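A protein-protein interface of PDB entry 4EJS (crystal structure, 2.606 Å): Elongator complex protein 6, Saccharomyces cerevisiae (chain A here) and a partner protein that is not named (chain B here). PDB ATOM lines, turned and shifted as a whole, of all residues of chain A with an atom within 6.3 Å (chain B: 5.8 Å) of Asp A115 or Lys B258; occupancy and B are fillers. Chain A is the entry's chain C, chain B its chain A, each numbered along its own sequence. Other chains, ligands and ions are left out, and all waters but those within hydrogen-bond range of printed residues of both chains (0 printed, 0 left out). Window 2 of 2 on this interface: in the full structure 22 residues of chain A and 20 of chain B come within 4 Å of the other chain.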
ATOM      1  N   GLU A  89     -13.618 -12.176   5.102  1.00  0.00           N
ATOM      2  CA  GLU A  89     -12.314 -12.099   4.430  1.00  0.00           C
ATOM      3  C   GLU A  89     -12.313 -11.033   3.335  1.00  0.00           C
ATOM      4  O   GLU A  89     -13.365 -10.621   2.833  1.00  0.00           O
ATOM      5  CB  GLU A  89     -11.898 -13.437   3.792  1.00  0.00           C
ATOM      6  CG  GLU A  89     -12.944 -14.524   3.833  1.00  0.00           C
ATOM      7  CD  GLU A  89     -14.233 -14.205   3.080  1.00  0.00           C
ATOM      8  OE1 GLU A  89     -14.254 -14.392   1.838  1.00  0.00           O
ATOM      9  OE2 GLU A  89     -15.227 -13.816   3.748  1.00  0.00           O
ATOM     10  N   ASP A 111      -7.822  -7.538   6.633  1.00  0.00           N
ATOM     11  CA  ASP A 111      -8.541  -8.772   6.919  1.00  0.00           C
ATOM     12  C   ASP A 111      -8.246  -9.288   8.328  1.00  0.00           C
ATOM     13  O   ASP A 111      -7.142  -9.745   8.617  1.00  0.00           O
ATOM     14  CB  ASP A 111      -8.181  -9.828   5.867  1.00  0.00           C
ATOM     15  CG  ASP A 111      -9.030 -11.085   5.976  1.00  0.00           C
ATOM     16  OD1 ASP A 111      -9.622 -11.312   7.056  1.00  0.00           O
ATOM     17  OD2 ASP A 111      -9.099 -11.845   4.976  1.00  0.00           O
ATOM     18  N   LEU A 113     -10.219 -11.682   9.703  1.00  0.00           N
ATOM     19  CA  LEU A 113     -10.782 -13.021   9.804  1.00  0.00           C
ATOM     20  C   LEU A 113      -9.679 -14.040   9.491  1.00  0.00           C
ATOM     21  O   LEU A 113      -9.375 -14.908  10.307  1.00  0.00           O
ATOM     22  CB  LEU A 113     -11.961 -13.218   8.846  1.00  0.00           C
ATOM     23  CG  LEU A 113     -12.387 -14.690   8.697  1.00  0.00           C
ATOM     24  CD1 LEU A 113     -13.041 -15.235   9.976  1.00  0.00           C
ATOM     25  CD2 LEU A 113     -13.299 -14.894   7.496  1.00  0.00           C
ATOM     26  N   SER A 114      -9.072 -13.912   8.312  1.00  0.00           N
ATOM     27  CA  SER A 114      -8.059 -14.863   7.836  1.00  0.00           C
ATOM     28  C   SER A 114      -6.841 -15.038   8.753  1.00  0.00           C
ATOM     29  O   SER A 114      -6.029 -14.124   8.916  1.00  0.00           O
ATOM     30  CB  SER A 114      -7.598 -14.482   6.426  1.00  0.00           C
ATOM     31  OG  SER A 114      -8.690 -14.536   5.515  1.00  0.00           O
ATOM     32  N   ASP A 115      -6.730 -16.228   9.338  1.00  0.00           N
ATOM     33  CA  ASP A 115      -5.620 -16.585  10.220  1.00  0.00           C
ATOM     34  C   ASP A 115      -5.512 -15.645  11.413  1.00  0.00           C
ATOM     35  O   ASP A 115      -4.473 -15.566  12.065  1.00  0.00           O
ATOM     36  CB  ASP A 115      -4.288 -16.602   9.453  1.00  0.00           C
ATOM     37  CG  ASP A 115      -4.329 -17.482   8.218  1.00  0.00           C
ATOM     38  OD1 ASP A 115      -4.790 -18.637   8.319  1.00  0.00           O
ATOM     39  OD2 ASP A 115      -3.911 -17.015   7.136  1.00  0.00           O
ATOM     40  N   PHE A 116      -6.587 -14.933  11.710  1.00  0.00           N
ATOM     41  CA  PHE A 116      -6.533 -13.937  12.767  1.00  0.00           C
ATOM     42  C   PHE A 116      -6.376 -14.555  14.152  1.00  0.00           C
ATOM     43  O   PHE A 116      -5.500 -14.145  14.908  1.00  0.00           O
ATOM     44  CB  PHE A 116      -7.736 -13.000  12.717  1.00  0.00           C
ATOM     45  CG  PHE A 116      -7.726 -11.977  13.799  1.00  0.00           C
ATOM     46  CD1 PHE A 116      -6.772 -10.971  13.804  1.00  0.00           C
ATOM     47  CD2 PHE A 116      -8.642 -12.035  14.835  1.00  0.00           C
ATOM     48  CE1 PHE A 116      -6.742 -10.022  14.810  1.00  0.00           C
ATOM     49  CE2 PHE A 116      -8.621 -11.089  15.852  1.00  0.00           C
ATOM     50  CZ  PHE A 116      -7.668 -10.076  15.835  1.00  0.00           C
ATOM     51  N   ILE A 117      -7.206 -15.548  14.480  1.00  0.00           N
ATOM     52  CA  ILE A 117      -7.088 -16.239  15.770  1.00  0.00           C
ATOM     53  C   ILE A 117      -5.714 -16.893  15.953  1.00  0.00           C
ATOM     54  O   ILE A 117      -5.083 -16.794  17.004  1.00  0.00           O
ATOM     55  CB  ILE A 117      -8.152 -17.350  15.929  1.00  0.00           C
ATOM     56  CG1 ILE A 117      -9.564 -16.771  15.940  1.00  0.00           C
ATOM     57  CG2 ILE A 117      -7.925 -18.091  17.208  1.00  0.00           C
ATOM     58  CD1 ILE A 117      -9.855 -15.912  17.135  1.00  0.00           C
ATOM     59  N   VAL A 118      -5.262 -17.568  14.907  1.00  0.00           N
ATOM     60  CA  VAL A 118      -4.059 -18.386  14.963  1.00  0.00           C
ATOM     61  C   VAL A 118      -2.765 -17.575  14.975  1.00  0.00           C
ATOM     62  O   VAL A 118      -1.825 -17.916  15.683  1.00  0.00           O
ATOM     63  CB  VAL A 118      -4.046 -19.389  13.792  1.00  0.00           C
ATOM     64  CG1 VAL A 118      -2.664 -19.846  13.520  1.00  0.00           C
ATOM     65  CG2 VAL A 118      -4.983 -20.558  14.100  1.00  0.00           C
ATOM     66  N   ASN A 119      -2.724 -16.495  14.203  1.00  0.00           N
ATOM     67  CA  ASN A 119      -1.532 -15.661  14.133  1.00  0.00           C
ATOM     68  C   ASN A 119      -1.524 -14.489  15.100  1.00  0.00           C
ATOM     69  O   ASN A 119      -0.471 -14.104  15.600  1.00  0.00           O
ATOM     70  CB  ASN A 119      -1.318 -15.138  12.712  1.00  0.00           C
ATOM     71  CG  ASN A 119      -1.003 -16.243  11.727  1.00  0.00           C
ATOM     72  OD1 ASN A 119      -1.204 -16.082  10.524  1.00  0.00           O
ATOM     73  ND2 ASN A 119      -0.516 -17.381  12.234  1.00  0.00           N
ATOM     74  N   ASN A 120      -2.695 -13.923  15.374  1.00  0.00           N
ATOM     75  CA  ASN A 120      -2.755 -12.665  16.114  1.00  0.00           C
ATOM     76  C   ASN A 120      -3.356 -12.686  17.520  1.00  0.00           C
ATOM     77  O   ASN A 120      -3.262 -11.696  18.248  1.00  0.00           O
ATOM     78  CB  ASN A 120      -3.437 -11.604  15.255  1.00  0.00           C
ATOM     79  CG  ASN A 120      -2.642 -11.301  14.023  1.00  0.00           C
ATOM     80  OD1 ASN A 120      -1.433 -11.084  14.110  1.00  0.00           O
ATOM     81  ND2 ASN A 120      -3.287 -11.334  12.862  1.00  0.00           N
ATOM     82  N   ILE A 121      -3.958 -13.800  17.914  1.00  0.00           N
ATOM     83  CA  ILE A 121      -4.616 -13.846  19.212  1.00  0.00           C
ATOM     84  C   ILE A 121      -4.008 -14.873  20.147  1.00  0.00           C
ATOM     85  O   ILE A 121      -3.903 -14.630  21.350  1.00  0.00           O
ATOM     86  CB  ILE A 121      -6.166 -14.035  19.081  1.00  0.00           C
ATOM     87  CG1 ILE A 121      -6.791 -12.767  18.507  1.00  0.00           C
ATOM     88  CG2 ILE A 121      -6.817 -14.351  20.438  1.00  0.00           C
ATOM     89  CD1 ILE A 121      -8.247 -12.747  18.590  1.00  0.00           C
ATOM     90  N   GLU B 211      -6.327 -27.471   9.368  1.00  0.00           N
ATOM     91  CA  GLU B 211      -5.474 -26.892   8.331  1.00  0.00           C
ATOM     92  C   GLU B 211      -4.654 -28.008   7.707  1.00  0.00           C
ATOM     93  O   GLU B 211      -4.748 -28.271   6.508  1.00  0.00           O
ATOM     94  CB  GLU B 211      -4.509 -25.866   8.930  1.00  0.00           C
ATOM     95  CG  GLU B 211      -4.804 -24.395   8.640  1.00  0.00           C
ATOM     96  CD  GLU B 211      -4.224 -23.907   7.320  1.00  0.00           C
ATOM     97  OE1 GLU B 211      -3.968 -24.760   6.450  1.00  0.00           O
ATOM     98  OE2 GLU B 211      -4.028 -22.679   7.149  1.00  0.00           O
ATOM     99  N   ARG B 253     -14.178 -20.941  10.495  1.00  0.00           N
ATOM    100  CA  ARG B 253     -14.762 -20.101   9.451  1.00  0.00           C
ATOM    101  C   ARG B 253     -13.667 -19.495   8.559  1.00  0.00           C
ATOM    102  O   ARG B 253     -13.826 -19.388   7.347  1.00  0.00           O
ATOM    103  CB  ARG B 253     -15.643 -19.000  10.056  1.00  0.00           C
ATOM    104  CG  ARG B 253     -15.942 -17.859   9.087  1.00  0.00           C
ATOM    105  CD  ARG B 253     -16.781 -16.803   9.734  1.00  0.00           C
ATOM    106  NE  ARG B 253     -17.140 -15.748   8.798  1.00  0.00           N
ATOM    107  CZ  ARG B 253     -18.201 -15.787   8.004  1.00  0.00           C
ATOM    108  NH1 ARG B 253     -19.012 -16.829   8.033  1.00  0.00           N
ATOM    109  NH2 ARG B 253     -18.442 -14.790   7.173  1.00  0.00           N
ATOM    110  N   SER B 254     -12.551 -19.119   9.172  1.00  0.00           N
ATOM    111  CA  SER B 254     -11.414 -18.565   8.453  1.00  0.00           C
ATOM    112  C   SER B 254     -10.829 -19.536   7.420  1.00  0.00           C
ATOM    113  O   SER B 254     -10.391 -19.121   6.341  1.00  0.00           O
ATOM    114  CB  SER B 254     -10.339 -18.171   9.448  1.00  0.00           C
ATOM    115  OG  SER B 254      -9.101 -18.055   8.798  1.00  0.00           O
ATOM    116  N   LEU B 255     -10.817 -20.824   7.760  1.00  0.00           N
ATOM    117  CA  LEU B 255     -10.317 -21.870   6.866  1.00  0.00           C
ATOM    118  C   LEU B 255     -11.305 -22.140   5.744  1.00  0.00           C
ATOM    119  O   LEU B 255     -10.924 -22.355   4.598  1.00  0.00           O
ATOM    120  CB  LEU B 255     -10.098 -23.165   7.642  1.00  0.00           C
ATOM    121  CG  LEU B 255      -8.930 -23.186   8.613  1.00  0.00           C
ATOM    122  CD1 LEU B 255      -8.961 -24.480   9.444  1.00  0.00           C
ATOM    123  CD2 LEU B 255      -7.633 -23.038   7.816  1.00  0.00           C
ATOM    124  N   VAL B 256     -12.587 -22.143   6.087  1.00  0.00           N
ATOM    125  CA  VAL B 256     -13.629 -22.351   5.097  1.00  0.00           C
ATOM    126  C   VAL B 256     -13.553 -21.287   4.001  1.00  0.00           C
ATOM    127  O   VAL B 256     -13.703 -21.614   2.824  1.00  0.00           O
ATOM    128  CB  VAL B 256     -15.029 -22.381   5.750  1.00  0.00           C
ATOM    129  CG1 VAL B 256     -16.121 -22.387   4.691  1.00  0.00           C
ATOM    130  CG2 VAL B 256     -15.158 -23.597   6.660  1.00  0.00           C
ATOM    131  N   LYS B 257     -13.317 -20.025   4.385  1.00  0.00           N
ATOM    132  CA  LYS B 257     -13.199 -18.925   3.410  1.00  0.00           C
ATOM    133  C   LYS B 257     -11.837 -18.932   2.708  1.00  0.00           C
ATOM    134  O   LYS B 257     -11.733 -18.556   1.538  1.00  0.00           O
ATOM    135  CB  LYS B 257     -13.412 -17.544   4.049  1.00  0.00           C
ATOM    136  CG  LYS B 257     -14.740 -17.322   4.748  1.00  0.00           C
ATOM    137  CD  LYS B 257     -15.892 -17.786   3.903  1.00  0.00           C
ATOM    138  CE  LYS B 257     -17.188 -17.689   4.679  1.00  0.00           C
ATOM    139  NZ  LYS B 257     -18.371 -17.673   3.775  1.00  0.00           N
ATOM    140  N   LYS B 258     -10.804 -19.358   3.429  1.00  0.00           N
ATOM    141  CA  LYS B 258      -9.446 -19.432   2.890  1.00  0.00           C
ATOM    142  C   LYS B 258      -9.313 -20.485   1.779  1.00  0.00           C
ATOM    143  O   LYS B 258      -8.646 -20.256   0.780  1.00  0.00           O
ATOM    144  CB  LYS B 258      -8.455 -19.694   4.021  1.00  0.00           C
ATOM    145  CG  LYS B 258      -6.993 -19.616   3.629  1.00  0.00           C
ATOM    146  CD  LYS B 258      -6.162 -20.103   4.787  1.00  0.00           C
ATOM    147  CE  LYS B 258      -4.708 -19.764   4.647  1.00  0.00           C
ATOM    148  NZ  LYS B 258      -4.005 -20.044   5.936  1.00  0.00           N
ATOM    149  N   TYR B 259      -9.965 -21.631   1.953  1.00  0.00           N
ATOM    150  CA  TYR B 259      -9.987 -22.664   0.928  1.00  0.00           C
ATOM    151  C   TYR B 259     -11.394 -22.775   0.389  1.00  0.00           C
ATOM    152  O   TYR B 259     -11.936 -23.868   0.264  1.00  0.00           O
ATOM    153  CB  TYR B 259      -9.523 -24.013   1.502  1.00  0.00           C
ATOM    154  CG  TYR B 259      -8.166 -23.929   2.165  1.00  0.00           C
ATOM    155  CD1 TYR B 259      -6.992 -24.140   1.439  1.00  0.00           C
ATOM    156  CD2 TYR B 259      -8.054 -23.615   3.514  1.00  0.00           C
ATOM    157  CE1 TYR B 259      -5.737 -24.049   2.052  1.00  0.00           C
ATOM    158  CE2 TYR B 259      -6.808 -23.525   4.138  1.00  0.00           C
ATOM    159  CZ  TYR B 259      -5.657 -23.741   3.402  1.00  0.00           C
ATOM    160  OH  TYR B 259      -4.430 -23.639   4.023  1.00  0.00           O
ATOM    161  N   TYR B 260     -11.985 -21.627   0.080  1.00  0.00           N
ATOM    162  CA  TYR B 260     -13.355 -21.560  -0.418  1.00  0.00           C
ATOM    163  C   TYR B 260     -13.491 -22.341  -1.717  1.00  0.00           C
ATOM    164  O   TYR B 260     -14.593 -22.719  -2.141  1.00  0.00           O
ATOM    165  CB  TYR B 260     -13.701 -20.115  -0.692  1.00  0.00           C
ATOM    166  CG  TYR B 260     -12.903 -19.521  -1.834  1.00  0.00           C
ATOM    167  CD1 TYR B 260     -13.455 -19.411  -3.117  1.00  0.00           C
ATOM    168  CD2 TYR B 260     -11.600 -19.062  -1.634  1.00  0.00           C
ATOM    169  CE1 TYR B 260     -12.730 -18.856  -4.165  1.00  0.00           C
ATOM    170  CE2 TYR B 260     -10.870 -18.502  -2.672  1.00  0.00           C
ATOM    171  CZ  TYR B 260     -11.438 -18.403  -3.939  1.00  0.00           C
ATOM    172  OH  TYR B 260     -10.714 -17.848  -4.980  1.00  0.00           O
ATOM    173  N   GLU B 261     -12.346 -22.546  -2.352  1.00  0.00           N
ATOM    174  CA  GLU B 261     -12.234 -23.348  -3.559  1.00  0.00           C
ATOM    175  C   GLU B 261     -12.828 -24.763  -3.381  1.00  0.00           C
ATOM    176  O   GLU B 261     -13.489 -25.271  -4.280  1.00  0.00           O
ATOM    177  CB  GLU B 261     -10.755 -23.412  -3.968  1.00  0.00           C
ATOM    178  CG  GLU B 261      -9.819 -23.859  -2.820  1.00  0.00           C
ATOM    179  CD  GLU B 261      -8.633 -22.919  -2.570  1.00  0.00           C
ATOM    180  OE1 GLU B 261      -8.819 -21.679  -2.594  1.00  0.00           O
ATOM    181  OE2 GLU B 261      -7.512 -23.431  -2.335  1.00  0.00           O
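The side-chain carboxylate (OE2) of Glu B211 is in salt-bridge range of the side-chain amino group (NZ) of Lys B258 (2.9 Å). The side-chain carboxylate (OD1) of Asp A111 sits at hydrogen-bond distance from the backbone NH (N) of Leu A113 (2.7 Å). OD2 of Asp A111 lies within hydrogen-bond range of OG of Ser A114.
Of chain B, only Ser B254 and Lys B258 come within 4 Å of Asp A115. Of the printed residues of chain B, Leu A113 touches Ser B254 (3.5 Å) and Lys B257 (3.9 Å). Of the printed residues of chain A, Ser B254 touches Leu A113 (3.5 Å), Ser A114 (3.5 Å) and Asp A115 (3.0 Å). Ile A117 touches none of the printed residues of chain B. Tyr B260 touches none of the printed residues of chain A. The nearest residue of chain B that does not touch Asp A115 is Glu B211 (4.3 Å).
Among the printed residues, merely in contact across the chains: Glu A89 with Lys B257 (3.1 Å), Ser A114 with Ser B254 (3.5 Å), Leu A113 with Ser B254 (3.5 Å) and Leu A113 with Lys B257 (3.9 Å).
OG of Ser B254 is in hydrogen-bond range of N of Asp A115, at 3.0 Å. OD1 of Asp A115 lies within salt-bridge range of NZ of Lys B258 (2.9 Å).
Of the 11 printed residues of chain A, 4 touch a printed residue of chain B. Along chain A the printed residues that touch a printed residue of chain B span positions 89 to 115. Of the 10 printed residues of chain B, 3 touch a printed residue of chain A. Printed residues of chain B that touch a printed residue of chain A: Ser B254, Lys B257 and Lys B258. Among the printed residues, 6 pairs touch across the chains.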
